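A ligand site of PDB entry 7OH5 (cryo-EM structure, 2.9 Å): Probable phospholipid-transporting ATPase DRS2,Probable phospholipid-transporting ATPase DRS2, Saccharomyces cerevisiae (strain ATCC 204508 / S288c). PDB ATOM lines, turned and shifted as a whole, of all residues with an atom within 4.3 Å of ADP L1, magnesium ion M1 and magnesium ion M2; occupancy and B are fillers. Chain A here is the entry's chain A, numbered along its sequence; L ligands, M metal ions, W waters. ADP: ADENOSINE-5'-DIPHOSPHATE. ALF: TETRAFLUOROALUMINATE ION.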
ATOM      1  N   ASP A 560     -13.229  -2.006  38.697  1.00  0.00           N
ATOM      2  CA  ASP A 560     -12.533  -2.493  37.515  1.00  0.00           C
ATOM      3  C   ASP A 560     -11.053  -2.196  37.695  1.00  0.00           C
ATOM      4  O   ASP A 560     -10.679  -1.263  38.411  1.00  0.00           O
ATOM      5  CB  ASP A 560     -13.107  -1.848  36.242  1.00  0.00           C
ATOM      6  CG  ASP A 560     -12.118  -1.845  35.083  1.00  0.00           C
ATOM      7  OD1 ASP A 560     -11.750  -2.944  34.595  1.00  0.00           O
ATOM      8  OD2 ASP A 560     -11.718  -0.746  34.665  1.00  0.00           O
ATOM      9  N   LYS A 561     -10.203  -3.008  37.058  1.00  0.00           N
ATOM     10  CA  LYS A 561      -8.753  -2.895  37.254  1.00  0.00           C
ATOM     11  C   LYS A 561      -8.135  -1.878  36.291  1.00  0.00           C
ATOM     12  O   LYS A 561      -7.646  -0.829  36.721  1.00  0.00           O
ATOM     13  CB  LYS A 561      -8.097  -4.268  37.100  1.00  0.00           C
ATOM     14  CG  LYS A 561      -6.633  -4.287  37.502  1.00  0.00           C
ATOM     15  CD  LYS A 561      -5.936  -5.554  37.063  1.00  0.00           C
ATOM     16  CE  LYS A 561      -5.797  -5.609  35.551  1.00  0.00           C
ATOM     17  NZ  LYS A 561      -5.030  -6.809  35.106  1.00  0.00           N
ATOM     18  N   THR A 562      -8.148  -2.186  34.999  1.00  0.00           N
ATOM     19  CA  THR A 562      -7.435  -1.384  34.016  1.00  0.00           C
ATOM     20  C   THR A 562      -8.105  -0.018  33.857  1.00  0.00           C
ATOM     21  O   THR A 562      -9.263   0.071  33.458  1.00  0.00           O
ATOM     22  CB  THR A 562      -7.392  -2.102  32.679  1.00  0.00           C
ATOM     23  OG1 THR A 562      -6.698  -3.349  32.822  1.00  0.00           O
ATOM     24  CG2 THR A 562      -6.676  -1.255  31.634  1.00  0.00           C
ATOM     25  N   GLY A 563      -7.375   1.036  34.174  1.00  0.00           N
ATOM     26  CA  GLY A 563      -7.885   2.390  34.053  1.00  0.00           C
ATOM     27  C   GLY A 563      -8.554   2.929  35.298  1.00  0.00           C
ATOM     28  O   GLY A 563      -8.300   4.062  35.702  1.00  0.00           O
ATOM     29  N   THR A 564      -9.421   2.121  35.908  1.00  0.00           N
ATOM     30  CA  THR A 564     -10.095   2.537  37.132  1.00  0.00           C
ATOM     31  C   THR A 564      -9.165   2.473  38.332  1.00  0.00           C
ATOM     32  O   THR A 564      -9.097   3.416  39.130  1.00  0.00           O
ATOM     33  CB  THR A 564     -11.340   1.681  37.364  1.00  0.00           C
ATOM     34  OG1 THR A 564     -12.214   1.774  36.235  1.00  0.00           O
ATOM     35  CG2 THR A 564     -12.075   2.130  38.618  1.00  0.00           C
ATOM     36  N   SER A 652      -5.716   1.786  21.991  1.00  0.00           N
ATOM     37  CA  SER A 652      -5.479   1.045  23.210  1.00  0.00           C
ATOM     38  C   SER A 652      -4.082   1.341  23.725  1.00  0.00           C
ATOM     39  O   SER A 652      -3.122   1.291  22.945  1.00  0.00           O
ATOM     40  CB  SER A 652      -5.633  -0.453  22.980  1.00  0.00           C
ATOM     41  OG  SER A 652      -5.459  -1.178  24.180  1.00  0.00           O
ATOM     42  N   ASP A 654      -2.027  -0.357  25.455  1.00  0.00           N
ATOM     43  CA  ASP A 654      -1.079  -1.461  25.326  1.00  0.00           C
ATOM     44  C   ASP A 654      -0.665  -1.680  23.874  1.00  0.00           C
ATOM     45  O   ASP A 654       0.377  -2.290  23.620  1.00  0.00           O
ATOM     46  CB  ASP A 654      -1.677  -2.742  25.916  1.00  0.00           C
ATOM     47  CG  ASP A 654      -2.988  -3.129  25.282  1.00  0.00           C
ATOM     48  OD1 ASP A 654      -3.484  -2.382  24.420  1.00  0.00           O
ATOM     49  OD2 ASP A 654      -3.529  -4.192  25.651  1.00  0.00           O
ATOM     50  N   GLU A 655      -1.464  -1.205  22.925  1.00  0.00           N
ATOM     51  CA  GLU A 655      -1.047  -1.238  21.531  1.00  0.00           C
ATOM     52  C   GLU A 655       0.200  -0.381  21.312  1.00  0.00           C
ATOM     53  O   GLU A 655       1.175  -0.825  20.695  1.00  0.00           O
ATOM     54  CB  GLU A 655      -2.185  -0.756  20.622  1.00  0.00           C
ATOM     55  CG  GLU A 655      -3.319  -1.746  20.447  1.00  0.00           C
ATOM     56  CD  GLU A 655      -3.036  -2.791  19.389  1.00  0.00           C
ATOM     57  OE1 GLU A 655      -1.862  -3.192  19.229  1.00  0.00           O
ATOM     58  OE2 GLU A 655      -3.985  -3.219  18.708  1.00  0.00           O
ATOM     59  N   PHE A 698     -10.518  -5.690  17.457  1.00  0.00           N
ATOM     60  CA  PHE A 698     -10.506  -6.287  18.792  1.00  0.00           C
ATOM     61  C   PHE A 698     -11.780  -5.921  19.528  1.00  0.00           C
ATOM     62  O   PHE A 698     -12.038  -4.740  19.784  1.00  0.00           O
ATOM     63  CB  PHE A 698      -9.278  -5.819  19.567  1.00  0.00           C
ATOM     64  CG  PHE A 698      -9.422  -5.943  21.056  1.00  0.00           C
ATOM     65  CD1 PHE A 698      -9.348  -7.176  21.678  1.00  0.00           C
ATOM     66  CD2 PHE A 698      -9.628  -4.819  21.842  1.00  0.00           C
ATOM     67  CE1 PHE A 698      -9.480  -7.300  23.051  1.00  0.00           C
ATOM     68  CE2 PHE A 698      -9.757  -4.934  23.214  1.00  0.00           C
ATOM     69  CZ  PHE A 698      -9.683  -6.168  23.822  1.00  0.00           C
ATOM     70  N   LYS A 703     -11.920 -10.629  22.891  1.00  0.00           N
ATOM     71  CA  LYS A 703     -10.685 -10.697  23.674  1.00  0.00           C
ATOM     72  C   LYS A 703      -9.492 -11.163  22.842  1.00  0.00           C
ATOM     73  O   LYS A 703      -8.572 -11.801  23.364  1.00  0.00           O
ATOM     74  CB  LYS A 703     -10.867 -11.599  24.902  1.00  0.00           C
ATOM     75  CG  LYS A 703     -12.033 -11.214  25.798  1.00  0.00           C
ATOM     76  CD  LYS A 703     -12.246 -12.242  26.900  1.00  0.00           C
ATOM     77  CE  LYS A 703     -11.102 -12.235  27.903  1.00  0.00           C
ATOM     78  NZ  LYS A 703     -11.060 -10.980  28.697  1.00  0.00           N
ATOM     79  N   ARG A 704      -9.492 -10.843  21.550  1.00  0.00           N
ATOM     80  CA  ARG A 704      -8.485 -11.367  20.640  1.00  0.00           C
ATOM     81  C   ARG A 704      -8.494 -10.552  19.359  1.00  0.00           C
ATOM     82  O   ARG A 704      -9.573 -10.266  18.810  1.00  0.00           O
ATOM     83  CB  ARG A 704      -8.753 -12.853  20.354  1.00  0.00           C
ATOM     84  CG  ARG A 704      -8.060 -13.411  19.137  1.00  0.00           C
ATOM     85  CD  ARG A 704      -8.309 -14.901  19.036  1.00  0.00           C
ATOM     86  NE  ARG A 704      -9.656 -15.256  19.479  1.00  0.00           N
ATOM     87  CZ  ARG A 704     -10.707 -15.344  18.677  1.00  0.00           C
ATOM     88  NH1 ARG A 704     -10.572 -15.120  17.377  1.00  0.00           N
ATOM     89  NH2 ARG A 704     -11.897 -15.665  19.160  1.00  0.00           N
ATOM     90  N   MET A 705      -7.306 -10.184  18.877  1.00  0.00           N
ATOM     91  CA  MET A 705      -7.142  -9.419  17.652  1.00  0.00           C
ATOM     92  C   MET A 705      -6.377 -10.237  16.629  1.00  0.00           C
ATOM     93  O   MET A 705      -5.385 -10.892  16.969  1.00  0.00           O
ATOM     94  CB  MET A 705      -6.411  -8.094  17.924  1.00  0.00           C
ATOM     95  CG  MET A 705      -5.909  -7.389  16.670  1.00  0.00           C
ATOM     96  SD  MET A 705      -5.124  -5.802  17.002  1.00  0.00           S
ATOM     97  CE  MET A 705      -6.540  -4.803  17.430  1.00  0.00           C
ATOM     98  N   LYS A 721      -3.198 -12.154  18.147  1.00  0.00           N
ATOM     99  CA  LYS A 721      -2.738 -11.847  19.482  1.00  0.00           C
ATOM    100  C   LYS A 721      -3.939 -11.601  20.382  1.00  0.00           C
ATOM    101  O   LYS A 721      -5.007 -11.199  19.905  1.00  0.00           O
ATOM    102  CB  LYS A 721      -1.795 -10.636  19.499  1.00  0.00           C
ATOM    103  CG  LYS A 721      -2.381  -9.377  18.881  1.00  0.00           C
ATOM    104  CD  LYS A 721      -1.393  -8.223  18.951  1.00  0.00           C
ATOM    105  CE  LYS A 721      -1.923  -6.991  18.252  1.00  0.00           C
ATOM    106  NZ  LYS A 721      -3.190  -6.502  18.860  1.00  0.00           N
ATOM    107  N   GLY A 722      -3.753 -11.841  21.671  1.00  0.00           N
ATOM    108  CA  GLY A 722      -4.853 -11.701  22.624  1.00  0.00           C
ATOM    109  C   GLY A 722      -4.502 -12.323  23.955  1.00  0.00           C
ATOM    110  O   GLY A 722      -3.323 -12.402  24.338  1.00  0.00           O
ATOM    111  N   ALA A 723      -5.532 -12.752  24.666  1.00  0.00           N
ATOM    112  CA  ALA A 723      -5.354 -13.376  25.969  1.00  0.00           C
ATOM    113  C   ALA A 723      -5.059 -14.871  25.809  1.00  0.00           C
ATOM    114  O   ALA A 723      -5.406 -15.493  24.800  1.00  0.00           O
ATOM    115  CB  ALA A 723      -6.580 -13.167  26.840  1.00  0.00           C
ATOM    116  N   ARG A 755       0.933  -6.916  32.790  1.00  0.00           N
ATOM    117  CA  ARG A 755      -0.160  -7.222  31.886  1.00  0.00           C
ATOM    118  C   ARG A 755       0.399  -7.982  30.682  1.00  0.00           C
ATOM    119  O   ARG A 755       1.181  -7.427  29.899  1.00  0.00           O
ATOM    120  CB  ARG A 755      -0.871  -5.943  31.462  1.00  0.00           C
ATOM    121  CG  ARG A 755      -2.220  -6.160  30.805  1.00  0.00           C
ATOM    122  CD  ARG A 755      -2.991  -4.849  30.703  1.00  0.00           C
ATOM    123  NE  ARG A 755      -4.350  -5.048  30.210  1.00  0.00           N
ATOM    124  CZ  ARG A 755      -4.690  -4.970  28.923  1.00  0.00           C
ATOM    125  NH1 ARG A 755      -3.777  -4.696  28.004  1.00  0.00           N
ATOM    126  NH2 ARG A 755      -5.947  -5.163  28.563  1.00  0.00           N
ATOM    127  N   THR A 756       0.009  -9.237  30.524  1.00  0.00           N
ATOM    128  CA  THR A 756       0.598 -10.133  29.553  1.00  0.00           C
ATOM    129  C   THR A 756      -0.348 -10.390  28.381  1.00  0.00           C
ATOM    130  O   THR A 756      -1.564 -10.242  28.501  1.00  0.00           O
ATOM    131  CB  THR A 756       0.993 -11.467  30.195  1.00  0.00           C
ATOM    132  OG1 THR A 756      -0.194 -12.188  30.543  1.00  0.00           O
ATOM    133  CG2 THR A 756       1.809 -11.226  31.450  1.00  0.00           C
ATOM    134  N   LEU A 757       0.237 -10.784  27.256  1.00  0.00           N
ATOM    135  CA  LEU A 757      -0.509 -11.161  26.060  1.00  0.00           C
ATOM    136  C   LEU A 757       0.147 -12.389  25.455  1.00  0.00           C
ATOM    137  O   LEU A 757       1.172 -12.883  25.931  1.00  0.00           O
ATOM    138  CB  LEU A 757      -0.563 -10.008  25.038  1.00  0.00           C
ATOM    139  CG  LEU A 757      -1.340  -8.740  25.384  1.00  0.00           C
ATOM    140  CD1 LEU A 757      -0.477  -7.748  26.146  1.00  0.00           C
ATOM    141  CD2 LEU A 757      -1.898  -8.112  24.119  1.00  0.00           C
ATOM    142  N   THR A 835     -12.645  -7.868  36.545  1.00  0.00           N
ATOM    143  CA  THR A 835     -11.587  -7.646  35.576  1.00  0.00           C
ATOM    144  C   THR A 835     -11.680  -8.670  34.455  1.00  0.00           C
ATOM    145  O   THR A 835     -11.990  -9.848  34.695  1.00  0.00           O
ATOM    146  CB  THR A 835     -10.211  -7.740  36.251  1.00  0.00           C
ATOM    147  OG1 THR A 835     -10.188  -6.881  37.389  1.00  0.00           O
ATOM    148  CG2 THR A 835      -9.117  -7.324  35.279  1.00  0.00           C
ATOM    149  N   GLY A 836     -11.411  -8.231  33.235  1.00  0.00           N
ATOM    150  CA  GLY A 836     -11.344  -9.111  32.084  1.00  0.00           C
ATOM    151  C   GLY A 836      -9.962  -9.643  31.771  1.00  0.00           C
ATOM    152  O   GLY A 836      -9.774 -10.254  30.716  1.00  0.00           O
ATOM    153  N   ASP A 837      -8.995  -9.438  32.654  1.00  0.00           N
ATOM    154  CA  ASP A 837      -7.623  -9.849  32.450  1.00  0.00           C
ATOM    155  C   ASP A 837      -7.352 -11.168  33.179  1.00  0.00           C
ATOM    156  O   ASP A 837      -8.295 -11.889  33.543  1.00  0.00           O
ATOM    157  CB  ASP A 837      -6.687  -8.714  32.904  1.00  0.00           C
ATOM    158  CG  ASP A 837      -5.314  -8.792  32.250  1.00  0.00           C
ATOM    159  OD1 ASP A 837      -5.150  -9.577  31.295  1.00  0.00           O
ATOM    160  OD2 ASP A 837      -4.406  -8.067  32.702  1.00  0.00           O
ATOM    161  N   ASP A 954     -14.373   2.346  33.331  1.00  0.00           N
ATOM    162  CA  ASP A 954     -14.019   3.130  32.152  1.00  0.00           C
ATOM    163  C   ASP A 954     -13.996   2.227  30.936  1.00  0.00           C
ATOM    164  O   ASP A 954     -13.665   1.042  31.032  1.00  0.00           O
ATOM    165  CB  ASP A 954     -12.663   3.828  32.327  1.00  0.00           C
ATOM    166  CG  ASP A 954     -11.515   2.850  32.475  1.00  0.00           C
ATOM    167  OD1 ASP A 954     -11.735   1.714  32.975  1.00  0.00           O
ATOM    168  OD2 ASP A 954     -10.384   3.205  32.107  1.00  0.00           O
ATOM    169  N   ASP A 958     -17.457  -1.952  30.326  1.00  0.00           N
ATOM    170  CA  ASP A 958     -18.261  -1.866  31.546  1.00  0.00           C
ATOM    171  C   ASP A 958     -19.293  -0.744  31.458  1.00  0.00           C
ATOM    172  O   ASP A 958     -19.541  -0.019  32.420  1.00  0.00           O
ATOM    173  CB  ASP A 958     -17.379  -1.682  32.773  1.00  0.00           C
ATOM    174  CG  ASP A 958     -16.394  -0.537  32.623  1.00  0.00           C
ATOM    175  OD1 ASP A 958     -16.815   0.631  32.658  1.00  0.00           O
ATOM    176  OD2 ASP A 958     -15.187  -0.818  32.483  1.00  0.00           O
HETATM  177  PB  ADP L   1      -9.275  -4.902  31.165  1.00  0.00           P
HETATM  178  O1B ADP L   1     -10.512  -4.418  31.828  1.00  0.00           O
HETATM  179  O2B ADP L   1      -8.203  -5.187  32.221  1.00  0.00           O
HETATM  180  O3B ADP L   1      -8.777  -3.860  30.217  1.00  0.00           O
HETATM  181  PA  ADP L   1     -10.119  -6.411  28.774  1.00  0.00           P
HETATM  182  O1A ADP L   1     -11.624  -6.186  28.731  1.00  0.00           O
HETATM  183  O2A ADP L   1      -9.431  -5.386  27.933  1.00  0.00           O
HETATM  184  O3A ADP L   1      -9.589  -6.316  30.318  1.00  0.00           O
HETATM  185  O5' ADP L   1      -9.779  -7.946  28.186  1.00  0.00           O
HETATM  186  C5' ADP L   1      -9.060  -8.064  26.941  1.00  0.00           C
HETATM  187  C4' ADP L   1      -7.776  -8.971  27.163  1.00  0.00           C
HETATM  188  O4' ADP L   1      -7.150  -9.311  25.778  1.00  0.00           O
HETATM  189  C3' ADP L   1      -6.900  -8.313  27.817  1.00  0.00           C
HETATM  190  O3' ADP L   1      -6.749  -8.863  29.157  1.00  0.00           O
HETATM  191  C2' ADP L   1      -5.462  -8.456  27.000  1.00  0.00           C
HETATM  192  O2' ADP L   1      -4.699  -9.580  27.510  1.00  0.00           O
HETATM  193  C1' ADP L   1      -5.754  -8.648  25.768  1.00  0.00           C
HETATM  194  N9  ADP L   1      -5.811  -7.338  25.050  1.00  0.00           N
HETATM  195  C8  ADP L   1      -5.862  -6.056  25.435  1.00  0.00           C
HETATM  196  N7  ADP L   1      -5.886  -5.313  24.292  1.00  0.00           N
HETATM  197  C5  ADP L   1      -5.845  -6.156  23.239  1.00  0.00           C
HETATM  198  C6  ADP L   1      -5.838  -5.950  21.874  1.00  0.00           C
HETATM  199  N6  ADP L   1      -5.882  -4.676  21.102  1.00  0.00           N
HETATM  200  N1  ADP L   1      -5.785  -7.014  21.016  1.00  0.00           N
HETATM  201  C2  ADP L   1      -5.736  -8.276  21.507  1.00  0.00           C
HETATM  202  N3  ADP L   1      -5.744  -8.483  22.858  1.00  0.00           N
HETATM  203  C4  ADP L   1      -5.788  -7.435  23.717  1.00  0.00           C
HETATM  204 AL   ALF L   2     -11.312  -3.574  33.072  1.00  0.00          AL
HETATM  205  F1  ALF L   2     -10.231  -3.578  34.475  1.00  0.00           F
HETATM  206  F2  ALF L   2     -12.376  -3.564  31.610  1.00  0.00           F
HETATM  207  F3  ALF L   2     -11.960  -5.173  33.537  1.00  0.00           F
HETATM  208  F4  ALF L   2     -10.658  -1.980  32.586  1.00  0.00           F
HETATM  209 MG    MG M   1      -9.812  -3.558  27.072  1.00  0.00          MG
HETATM  210 MG    MG M   2     -11.131  -0.334  32.758  1.00  0.00          MG
HETATM  211  O   HOH W   1     -12.970  -0.809  32.049  1.00  0.00           O
HETATM  212  O   HOH W   2     -10.515   0.060  30.815  1.00  0.00           O
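An aluminium atom (AL) of ALF L2 is bound by the side-chain carboxylate of Asp 560 (1.7 Å).
The backbone NH (N) of Lys 561 lies within hydrogen-bond range of a fluorine (F1) of ALF L2, 2.6 Å away.
The side-chain carboxylate of Glu 655 lies within hydrogen-bond range of a nitrogen (N6) of ADP L1, at 3.4 Å.
N of Thr 562 is in hydrogen-bond range of F1 of ALF L2 (2.6 Å).
O3' of ADP L1 sits at hydrogen-bond distance from OD1 of Asp 837, 2.8 Å away.
The guanidinium group (NH2) of Arg 755 is in salt-bridge range of an oxygen (O3B) of ADP L1 (3.5 Å).
OG1 of Thr 562 sits at hydrogen-bond distance from O2B of ADP L1.
An oxygen (O5') of ADP L1 sits at hydrogen-bond distance from the side-chain amino group (NZ) of Lys 703, 3.3 Å away.
A nitrogen (N1) of ADP L1 is in hydrogen-bond range of the side-chain amino group (NZ) of Lys 721.
N of Gly 836 lies within hydrogen-bond range of F3 of ALF L2 (3.1 Å).
The backbone carbonyl oxygen (O) of Thr 756 sits at hydrogen-bond distance from an oxygen (O2') of ADP L1.
An oxygen (O1B) of ADP L1 binds an aluminium atom (AL) of ALF L2 (1.7 Å).
The side-chain carboxylate (OE2) of Glu 655 lies within salt-bridge range of the side-chain amino group (NZ) of Lys 721 (3.4 Å).
N of Asp 954 sits at hydrogen-bond distance from OD1 of Asp 958 (3.1 Å).
OD2 of Asp 654 lies within salt-bridge range of NH1 of Arg 755.
The backbone carbonyl oxygen of Lys 703 sits at hydrogen-bond distance from the backbone NH of Ala 723 (3.4 Å).
The side-chain carboxylate (OD2) of Asp 837 lies within salt-bridge range of the side-chain amino group (NZ) of Lys 561.
NE of Arg 755 lies within salt-bridge range of OD2 of Asp 837, at 3.9 Å.
The side-chain hydroxyl (OG1) of Thr 564 lies close to the side-chain carboxylate (OD1) of Asp 954, 3.3 Å away.
The side-chain amino group of Lys 703 sits at hydrogen-bond distance from the backbone carbonyl oxygen of Gly 836, at 2.5 Å.
OD2 of Asp 654 lies close to N7 of ADP L1, at 2.9 Å.
An oxygen (O5') of ADP L1 lies close to the backbone carbonyl oxygen (O) of Gly 836 (3.4 Å).
Residues that only touch ADP L1: Phe 698 (3.6 Å), Met 705 (3.3 Å), Gly 722 (3.3 Å), Ala 723 (3.96 Å), Leu 757 (3.97 Å) and Thr 835 (3.8 Å).
Hydrophobic or aromatic side chains that line ADP L1: Phe 698, Met 705 and Leu 757.
No residue comes within 4 Å of magnesium ion M1.
The nearest printed residue that does not touch magnesium ion M1 is Phe 698 (4.1 Å).
Three residues have an atom within 4 Å of magnesium ion M2: Asp 560, Thr 562 and Asp 954.
The nearest printed residue that does not touch magnesium ion M2 is Asp 958 (4.1 Å).
Magnesium ion M1 is bound by O2A of ADP L1, 2.1 Å away.
Magnesium ion M2 is bound by F4 of ALF L2 (1.7 Å).
Water W1 is bound to magnesium ion M2, at 2.0 Å.
The backbone carbonyl oxygen (O) of Thr 562 is bound to magnesium ion M2 (2.0 Å).
The side-chain carboxylate (OD2) of Asp 560 binds magnesium ion M2 (2.0 Å).
Water W2 is bound to magnesium ion M2 (2.1 Å).
The side-chain carboxylate (OD1) of Asp 954 binds magnesium ion M2, at 2.1 Å.
Magnesium ion M2 has six donor atoms within binding distance.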
